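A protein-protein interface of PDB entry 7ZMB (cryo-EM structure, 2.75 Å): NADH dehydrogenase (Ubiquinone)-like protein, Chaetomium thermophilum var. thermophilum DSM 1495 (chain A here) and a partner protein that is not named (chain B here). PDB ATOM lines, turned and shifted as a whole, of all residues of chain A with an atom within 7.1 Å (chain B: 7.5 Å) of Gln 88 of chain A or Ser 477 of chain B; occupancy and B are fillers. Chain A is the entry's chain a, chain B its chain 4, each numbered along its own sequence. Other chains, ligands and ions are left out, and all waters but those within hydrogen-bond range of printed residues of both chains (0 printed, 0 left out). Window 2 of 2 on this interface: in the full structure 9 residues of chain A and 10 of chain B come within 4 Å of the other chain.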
ATOM      1  N   TRP A  84      21.001 -25.544 -24.758  1.00  0.00           N
ATOM      2  CA  TRP A  84      20.716 -24.146 -25.044  1.00  0.00           C
ATOM      3  C   TRP A  84      21.303 -23.275 -23.953  1.00  0.00           C
ATOM      4  O   TRP A  84      21.207 -23.602 -22.766  1.00  0.00           O
ATOM      5  CB  TRP A  84      19.220 -23.884 -25.141  1.00  0.00           C
ATOM      6  CG  TRP A  84      18.556 -24.641 -26.231  1.00  0.00           C
ATOM      7  CD1 TRP A  84      17.590 -25.584 -26.096  1.00  0.00           C
ATOM      8  CD2 TRP A  84      18.813 -24.523 -27.628  1.00  0.00           C
ATOM      9  NE1 TRP A  84      17.222 -26.063 -27.324  1.00  0.00           N
ATOM     10  CE2 TRP A  84      17.963 -25.426 -28.284  1.00  0.00           C
ATOM     11  CE3 TRP A  84      19.676 -23.733 -28.391  1.00  0.00           C
ATOM     12  CZ2 TRP A  84      17.950 -25.564 -29.666  1.00  0.00           C
ATOM     13  CZ3 TRP A  84      19.666 -23.876 -29.759  1.00  0.00           C
ATOM     14  CH2 TRP A  84      18.809 -24.784 -30.385  1.00  0.00           C
ATOM     15  N   TRP A  85      21.918 -22.166 -24.359  1.00  0.00           N
ATOM     16  CA  TRP A  85      22.319 -21.165 -23.381  1.00  0.00           C
ATOM     17  C   TRP A  85      21.105 -20.612 -22.659  1.00  0.00           C
ATOM     18  O   TRP A  85      21.124 -20.440 -21.436  1.00  0.00           O
ATOM     19  CB  TRP A  85      23.099 -20.044 -24.059  1.00  0.00           C
ATOM     20  CG  TRP A  85      23.263 -18.856 -23.188  1.00  0.00           C
ATOM     21  CD1 TRP A  85      24.153 -18.703 -22.170  1.00  0.00           C
ATOM     22  CD2 TRP A  85      22.501 -17.650 -23.242  1.00  0.00           C
ATOM     23  NE1 TRP A  85      24.001 -17.470 -21.591  1.00  0.00           N
ATOM     24  CE2 TRP A  85      22.990 -16.803 -22.230  1.00  0.00           C
ATOM     25  CE3 TRP A  85      21.455 -17.202 -24.050  1.00  0.00           C
ATOM     26  CZ2 TRP A  85      22.468 -15.536 -22.006  1.00  0.00           C
ATOM     27  CZ3 TRP A  85      20.938 -15.944 -23.822  1.00  0.00           C
ATOM     28  CH2 TRP A  85      21.446 -15.126 -22.811  1.00  0.00           C
ATOM     29  N   ASP A  86      20.037 -20.334 -23.397  1.00  0.00           N
ATOM     30  CA  ASP A  86      18.755 -19.921 -22.838  1.00  0.00           C
ATOM     31  C   ASP A  86      17.746 -20.989 -23.239  1.00  0.00           C
ATOM     32  O   ASP A  86      17.163 -20.936 -24.323  1.00  0.00           O
ATOM     33  CB  ASP A  86      18.347 -18.528 -23.330  1.00  0.00           C
ATOM     34  CG  ASP A  86      17.041 -18.043 -22.716  1.00  0.00           C
ATOM     35  OD1 ASP A  86      16.487 -18.737 -21.837  1.00  0.00           O
ATOM     36  OD2 ASP A  86      16.572 -16.955 -23.108  1.00  0.00           O
ATOM     37  N   LYS A  87      17.561 -21.973 -22.357  1.00  0.00           N
ATOM     38  CA  LYS A  87      16.623 -23.055 -22.636  1.00  0.00           C
ATOM     39  C   LYS A  87      15.208 -22.524 -22.794  1.00  0.00           C
ATOM     40  O   LYS A  87      14.472 -22.949 -23.691  1.00  0.00           O
ATOM     41  CB  LYS A  87      16.685 -24.094 -21.516  1.00  0.00           C
ATOM     42  CG  LYS A  87      15.856 -25.337 -21.763  1.00  0.00           C
ATOM     43  CD  LYS A  87      15.982 -26.312 -20.605  1.00  0.00           C
ATOM     44  CE  LYS A  87      17.361 -26.951 -20.573  1.00  0.00           C
ATOM     45  NZ  LYS A  87      17.583 -27.840 -21.745  1.00  0.00           N
ATOM     46  N   GLN A  88      14.821 -21.578 -21.938  1.00  0.00           N
ATOM     47  CA  GLN A  88      13.488 -20.998 -21.990  1.00  0.00           C
ATOM     48  C   GLN A  88      13.185 -20.387 -23.350  1.00  0.00           C
ATOM     49  O   GLN A  88      12.016 -20.314 -23.742  1.00  0.00           O
ATOM     50  CB  GLN A  88      13.361 -19.947 -20.887  1.00  0.00           C
ATOM     51  CG  GLN A  88      11.990 -19.337 -20.720  1.00  0.00           C
ATOM     52  CD  GLN A  88      11.666 -19.061 -19.266  1.00  0.00           C
ATOM     53  OE1 GLN A  88      12.369 -18.306 -18.593  1.00  0.00           O
ATOM     54  NE2 GLN A  88      10.590 -19.663 -18.778  1.00  0.00           N
ATOM     55  N   GLU A  89      14.213 -19.972 -24.083  1.00  0.00           N
ATOM     56  CA  GLU A  89      14.059 -19.428 -25.422  1.00  0.00           C
ATOM     57  C   GLU A  89      14.486 -20.400 -26.514  1.00  0.00           C
ATOM     58  O   GLU A  89      14.085 -20.222 -27.666  1.00  0.00           O
ATOM     59  CB  GLU A  89      14.865 -18.122 -25.535  1.00  0.00           C
ATOM     60  CG  GLU A  89      14.782 -17.388 -26.862  1.00  0.00           C
ATOM     61  CD  GLU A  89      13.391 -16.870 -27.165  1.00  0.00           C
ATOM     62  OE1 GLU A  89      12.619 -16.630 -26.215  1.00  0.00           O
ATOM     63  OE2 GLU A  89      13.078 -16.689 -28.360  1.00  0.00           O
ATOM     64  N   ARG A  90      15.247 -21.440 -26.167  1.00  0.00           N
ATOM     65  CA  ARG A  90      15.840 -22.376 -27.124  1.00  0.00           C
ATOM     66  C   ARG A  90      16.740 -21.638 -28.102  1.00  0.00           C
ATOM     67  O   ARG A  90      16.599 -21.736 -29.320  1.00  0.00           O
ATOM     68  CB  ARG A  90      14.770 -23.178 -27.862  1.00  0.00           C
ATOM     69  CG  ARG A  90      13.839 -23.953 -26.945  1.00  0.00           C
ATOM     70  CD  ARG A  90      12.601 -24.298 -27.690  1.00  0.00           C
ATOM     71  NE  ARG A  90      11.822 -25.368 -27.090  1.00  0.00           N
ATOM     72  CZ  ARG A  90      10.827 -25.978 -27.720  1.00  0.00           C
ATOM     73  NH1 ARG A  90      10.522 -25.623 -28.959  1.00  0.00           N
ATOM     74  NH2 ARG A  90      10.135 -26.932 -27.121  1.00  0.00           N
ATOM     75  N   ARG A  91      17.679 -20.884 -27.548  1.00  0.00           N
ATOM     76  CA  ARG A  91      18.584 -20.078 -28.346  1.00  0.00           C
ATOM     77  C   ARG A  91      19.992 -20.191 -27.787  1.00  0.00           C
ATOM     78  O   ARG A  91      20.187 -20.204 -26.569  1.00  0.00           O
ATOM     79  CB  ARG A  91      18.132 -18.613 -28.371  1.00  0.00           C
ATOM     80  CG  ARG A  91      18.726 -17.805 -29.499  1.00  0.00           C
ATOM     81  CD  ARG A  91      18.514 -16.318 -29.298  1.00  0.00           C
ATOM     82  NE  ARG A  91      19.499 -15.546 -30.042  1.00  0.00           N
ATOM     83  CZ  ARG A  91      20.572 -14.986 -29.500  1.00  0.00           C
ATOM     84  NH1 ARG A  91      20.797 -15.091 -28.199  1.00  0.00           N
ATOM     85  NH2 ARG A  91      21.418 -14.310 -30.258  1.00  0.00           N
ATOM     86  N   MET A 106       9.922 -17.868 -28.611  1.00  0.00           N
ATOM     87  CA  MET A 106       9.013 -18.777 -27.918  1.00  0.00           C
ATOM     88  C   MET A 106       7.727 -18.075 -27.490  1.00  0.00           C
ATOM     89  O   MET A 106       6.642 -18.658 -27.577  1.00  0.00           O
ATOM     90  CB  MET A 106       9.713 -19.409 -26.718  1.00  0.00           C
ATOM     91  CG  MET A 106      10.829 -20.351 -27.102  1.00  0.00           C
ATOM     92  SD  MET A 106      10.300 -21.680 -28.184  1.00  0.00           S
ATOM     93  CE  MET A 106       9.341 -22.682 -27.050  1.00  0.00           C
ATOM     94  N   PHE A 107       7.822 -16.828 -27.028  1.00  0.00           N
ATOM     95  CA  PHE A 107       6.633 -16.042 -26.697  1.00  0.00           C
ATOM     96  C   PHE A 107       6.157 -15.305 -27.951  1.00  0.00           C
ATOM     97  O   PHE A 107       6.204 -14.081 -28.064  1.00  0.00           O
ATOM     98  CB  PHE A 107       6.910 -15.099 -25.535  1.00  0.00           C
ATOM     99  CG  PHE A 107       5.692 -14.363 -25.044  1.00  0.00           C
ATOM    100  CD1 PHE A 107       4.431 -14.905 -25.197  1.00  0.00           C
ATOM    101  CD2 PHE A 107       5.815 -13.160 -24.382  1.00  0.00           C
ATOM    102  CE1 PHE A 107       3.317 -14.241 -24.741  1.00  0.00           C
ATOM    103  CE2 PHE A 107       4.709 -12.498 -23.918  1.00  0.00           C
ATOM    104  CZ  PHE A 107       3.455 -13.040 -24.099  1.00  0.00           C
ATOM    105  N   ARG B 404      13.082  -9.798 -19.722  1.00  0.00           N
ATOM    106  CA  ARG B 404      12.207 -10.943 -19.569  1.00  0.00           C
ATOM    107  C   ARG B 404      12.097 -11.241 -18.083  1.00  0.00           C
ATOM    108  O   ARG B 404      13.095 -11.196 -17.362  1.00  0.00           O
ATOM    109  CB  ARG B 404      12.749 -12.149 -20.350  1.00  0.00           C
ATOM    110  CG  ARG B 404      11.948 -13.429 -20.247  1.00  0.00           C
ATOM    111  CD  ARG B 404      12.407 -14.281 -19.084  1.00  0.00           C
ATOM    112  NE  ARG B 404      13.790 -14.720 -19.208  1.00  0.00           N
ATOM    113  CZ  ARG B 404      14.272 -15.476 -20.189  1.00  0.00           C
ATOM    114  NH1 ARG B 404      13.487 -15.928 -21.153  1.00  0.00           N
ATOM    115  NH2 ARG B 404      15.554 -15.804 -20.188  1.00  0.00           N
ATOM    116  N   GLY B 405      10.878 -11.538 -17.641  1.00  0.00           N
ATOM    117  CA  GLY B 405      10.615 -11.892 -16.261  1.00  0.00           C
ATOM    118  C   GLY B 405      11.288 -11.042 -15.200  1.00  0.00           C
ATOM    119  O   GLY B 405      12.062 -11.560 -14.397  1.00  0.00           O
ATOM    120  N   LEU B 406      11.027  -9.740 -15.179  1.00  0.00           N
ATOM    121  CA  LEU B 406      11.541  -8.926 -14.090  1.00  0.00           C
ATOM    122  C   LEU B 406      10.693  -9.001 -12.836  1.00  0.00           C
ATOM    123  O   LEU B 406      11.153  -8.575 -11.773  1.00  0.00           O
ATOM    124  CB  LEU B 406      11.684  -7.461 -14.507  1.00  0.00           C
ATOM    125  CG  LEU B 406      12.757  -7.158 -15.534  1.00  0.00           C
ATOM    126  CD1 LEU B 406      12.708  -5.706 -15.925  1.00  0.00           C
ATOM    127  CD2 LEU B 406      14.097  -7.496 -14.939  1.00  0.00           C
ATOM    128  N   THR B 407       9.477  -9.535 -12.937  1.00  0.00           N
ATOM    129  CA  THR B 407       8.619  -9.692 -11.773  1.00  0.00           C
ATOM    130  C   THR B 407       9.264 -10.568 -10.708  1.00  0.00           C
ATOM    131  O   THR B 407       8.950 -10.421  -9.524  1.00  0.00           O
ATOM    132  CB  THR B 407       7.282 -10.276 -12.212  1.00  0.00           C
ATOM    133  OG1 THR B 407       6.668  -9.393 -13.148  1.00  0.00           O
ATOM    134  CG2 THR B 407       6.354 -10.438 -11.051  1.00  0.00           C
ATOM    135  N   GLN B 408      10.188 -11.454 -11.093  1.00  0.00           N
ATOM    136  CA  GLN B 408      10.862 -12.275 -10.098  1.00  0.00           C
ATOM    137  C   GLN B 408      11.801 -11.479  -9.209  1.00  0.00           C
ATOM    138  O   GLN B 408      12.155 -11.955  -8.128  1.00  0.00           O
ATOM    139  CB  GLN B 408      11.650 -13.408 -10.749  1.00  0.00           C
ATOM    140  CG  GLN B 408      10.824 -14.528 -11.299  1.00  0.00           C
ATOM    141  CD  GLN B 408      11.636 -15.779 -11.468  1.00  0.00           C
ATOM    142  OE1 GLN B 408      12.804 -15.724 -11.836  1.00  0.00           O
ATOM    143  NE2 GLN B 408      11.026 -16.921 -11.189  1.00  0.00           N
ATOM    144  N   ILE B 409      12.203 -10.286  -9.626  1.00  0.00           N
ATOM    145  CA  ILE B 409      13.300  -9.586  -8.972  1.00  0.00           C
ATOM    146  C   ILE B 409      12.849  -8.185  -8.578  1.00  0.00           C
ATOM    147  O   ILE B 409      13.374  -7.597  -7.626  1.00  0.00           O
ATOM    148  CB  ILE B 409      14.536  -9.569  -9.895  1.00  0.00           C
ATOM    149  CG1 ILE B 409      15.197 -10.933  -9.882  1.00  0.00           C
ATOM    150  CG2 ILE B 409      15.567  -8.564  -9.442  1.00  0.00           C
ATOM    151  CD1 ILE B 409      15.650 -11.356  -8.509  1.00  0.00           C
ATOM    152  N   ILE B 472       8.332  -7.926 -20.548  1.00  0.00           N
ATOM    153  CA  ILE B 472       9.306  -7.388 -19.599  1.00  0.00           C
ATOM    154  C   ILE B 472       9.082  -7.931 -18.196  1.00  0.00           C
ATOM    155  O   ILE B 472       9.997  -8.471 -17.574  1.00  0.00           O
ATOM    156  CB  ILE B 472       9.272  -5.847 -19.617  1.00  0.00           C
ATOM    157  CG1 ILE B 472       9.658  -5.334 -20.995  1.00  0.00           C
ATOM    158  CG2 ILE B 472      10.189  -5.273 -18.549  1.00  0.00           C
ATOM    159  CD1 ILE B 472       9.547  -3.867 -21.141  1.00  0.00           C
ATOM    160  N   ALA B 473       7.873  -7.783 -17.662  1.00  0.00           N
ATOM    161  CA  ALA B 473       7.616  -8.239 -16.302  1.00  0.00           C
ATOM    162  C   ALA B 473       7.506  -9.753 -16.234  1.00  0.00           C
ATOM    163  O   ALA B 473       8.011 -10.374 -15.294  1.00  0.00           O
ATOM    164  CB  ALA B 473       6.349  -7.582 -15.761  1.00  0.00           C
ATOM    165  N   PHE B 474       6.871 -10.365 -17.234  1.00  0.00           N
ATOM    166  CA  PHE B 474       6.551 -11.789 -17.236  1.00  0.00           C
ATOM    167  C   PHE B 474       7.297 -12.487 -18.361  1.00  0.00           C
ATOM    168  O   PHE B 474       8.259 -11.944 -18.907  1.00  0.00           O
ATOM    169  CB  PHE B 474       5.049 -12.034 -17.403  1.00  0.00           C
ATOM    170  CG  PHE B 474       4.213 -11.572 -16.254  1.00  0.00           C
ATOM    171  CD1 PHE B 474       4.780 -11.255 -15.035  1.00  0.00           C
ATOM    172  CD2 PHE B 474       2.841 -11.464 -16.392  1.00  0.00           C
ATOM    173  CE1 PHE B 474       3.989 -10.826 -13.984  1.00  0.00           C
ATOM    174  CE2 PHE B 474       2.051 -11.036 -15.345  1.00  0.00           C
ATOM    175  CZ  PHE B 474       2.627 -10.722 -14.142  1.00  0.00           C
ATOM    176  N   GLY B 475       6.888 -13.706 -18.686  1.00  0.00           N
ATOM    177  CA  GLY B 475       7.410 -14.385 -19.852  1.00  0.00           C
ATOM    178  C   GLY B 475       8.635 -15.220 -19.585  1.00  0.00           C
ATOM    179  O   GLY B 475       9.440 -15.445 -20.495  1.00  0.00           O
ATOM    180  N   GLY B 476       8.799 -15.692 -18.358  1.00  0.00           N
ATOM    181  CA  GLY B 476       9.992 -16.419 -17.994  1.00  0.00           C
ATOM    182  C   GLY B 476      10.541 -15.994 -16.656  1.00  0.00           C
ATOM    183  O   GLY B 476       9.948 -15.155 -15.978  1.00  0.00           O
ATOM    184  N   SER B 477      11.679 -16.560 -16.262  1.00  0.00           N
ATOM    185  CA  SER B 477      12.173 -16.348 -14.904  1.00  0.00           C
ATOM    186  C   SER B 477      12.859 -14.991 -14.769  1.00  0.00           C
ATOM    187  O   SER B 477      12.345 -14.097 -14.097  1.00  0.00           O
ATOM    188  CB  SER B 477      13.115 -17.493 -14.517  1.00  0.00           C
ATOM    189  OG  SER B 477      14.266 -17.507 -15.340  1.00  0.00           O
ATOM    190  N   VAL B 478      14.002 -14.815 -15.426  1.00  0.00           N
ATOM    191  CA  VAL B 478      14.605 -13.505 -15.647  1.00  0.00           C
ATOM    192  C   VAL B 478      15.374 -13.632 -16.944  1.00  0.00           C
ATOM    193  O   VAL B 478      15.736 -14.733 -17.367  1.00  0.00           O
ATOM    194  CB  VAL B 478      15.584 -12.991 -14.557  1.00  0.00           C
ATOM    195  CG1 VAL B 478      14.963 -12.951 -13.163  1.00  0.00           C
ATOM    196  CG2 VAL B 478      16.894 -13.747 -14.598  1.00  0.00           C
ATOM    197  N   SER B 479      15.615 -12.502 -17.590  1.00  0.00           N
ATOM    198  CA  SER B 479      16.445 -12.532 -18.778  1.00  0.00           C
ATOM    199  C   SER B 479      17.842 -13.018 -18.406  1.00  0.00           C
ATOM    200  O   SER B 479      18.442 -12.545 -17.439  1.00  0.00           O
ATOM    201  CB  SER B 479      16.492 -11.149 -19.416  1.00  0.00           C
ATOM    202  OG  SER B 479      17.327 -11.134 -20.552  1.00  0.00           O
ATOM    203  N   LEU B 480      18.349 -13.978 -19.167  1.00  0.00           N
ATOM    204  CA  LEU B 480      19.644 -14.570 -18.879  1.00  0.00           C
ATOM    205  C   LEU B 480      20.806 -13.718 -19.355  1.00  0.00           C
ATOM    206  O   LEU B 480      21.960 -14.094 -19.131  1.00  0.00           O
ATOM    207  CB  LEU B 480      19.741 -15.969 -19.492  1.00  0.00           C
ATOM    208  CG  LEU B 480      18.645 -16.931 -19.040  1.00  0.00           C
ATOM    209  CD1 LEU B 480      18.815 -18.270 -19.707  1.00  0.00           C
ATOM    210  CD2 LEU B 480      18.663 -17.080 -17.530  1.00  0.00           C
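The backbone NH (N) of Trp 85 of chain A lies within hydrogen-bond range of the backbone carbonyl oxygen (O) of Arg 91 of chain A (3.4 Å).
OD1 of Asp 86 of chain A lies close to N of Gln 88 of chain A (3.3 Å).
The backbone NH (N) of Asp 86 of chain A sits at hydrogen-bond distance from the backbone carbonyl oxygen (O) of Arg 91 of chain A (3.2 Å).
NE of Arg 404 of chain B is in hydrogen-bond range of O of Val 478 of chain B.
O of Arg 404 of chain B is in hydrogen-bond range of N of Ser 479 of chain B.
The backbone carbonyl oxygen of Ser 477 of chain B lies close to the side-chain amide oxygen of Gln 408 of chain B, at 2.8 Å.
Of the 15 printed residues of chain B, 4 touch a printed residue of chain A.
Hydrophobic or aromatic side chains of chain B that line the printed part of chain A: Leu 480.
Printed residues of chain A that touch a printed residue of chain B: Trp 85, Asp 86 and Gln 88.
Hydrophobic or aromatic side chains of chain A that line the printed part of chain B: Trp 85.
Among the printed residues, 6 pairs touch across the chains.
Among the printed residues, Asp or Glu carboxylates within 4 Å of a Lys or Arg side-chain nitrogen of the other chain: Asp 86 of chain A with Arg 404 of chain B.
Among the printed residues, merely in contact across the chains: Gln 88 of chain A with Gly 476 of chain B, Asp 86 of chain A with Leu 480 of chain B, Trp 85 of chain A with Leu 480 of chain B and Gln 88 of chain A with Arg 404 of chain B.
Gln 88 of chain A touches just these residues of chain B: Arg 404, Gly 476 and Ser 477.
Ser 477 of chain B touches one residue of chain A.
Printed residues of chain A within 4 Å of Arg 404 of chain B: Asp 86 and Gln 88.
Printed residues of chain B within 4 Å of Trp 85 of chain A: Leu 480 (3.3 Å).
Ile 409 of chain B touches none of the printed residues of chain A.
Glu 89 of chain A touches none of the printed residues of chain B.
The nearest printed residue of chain B that does not touch Asp 86 of chain A is Val 478 of chain B (6.0 Å).
The guanidinium group (NH2) of Arg 404 of chain B lies within salt-bridge range of the side-chain carboxylate (OD2) of Asp 86 of chain A, at 3.3 Å.
The side-chain amide oxygen (OE1) of Gln 88 of chain A is in hydrogen-bond range of the backbone NH (N) of Ser 477 of chain B.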
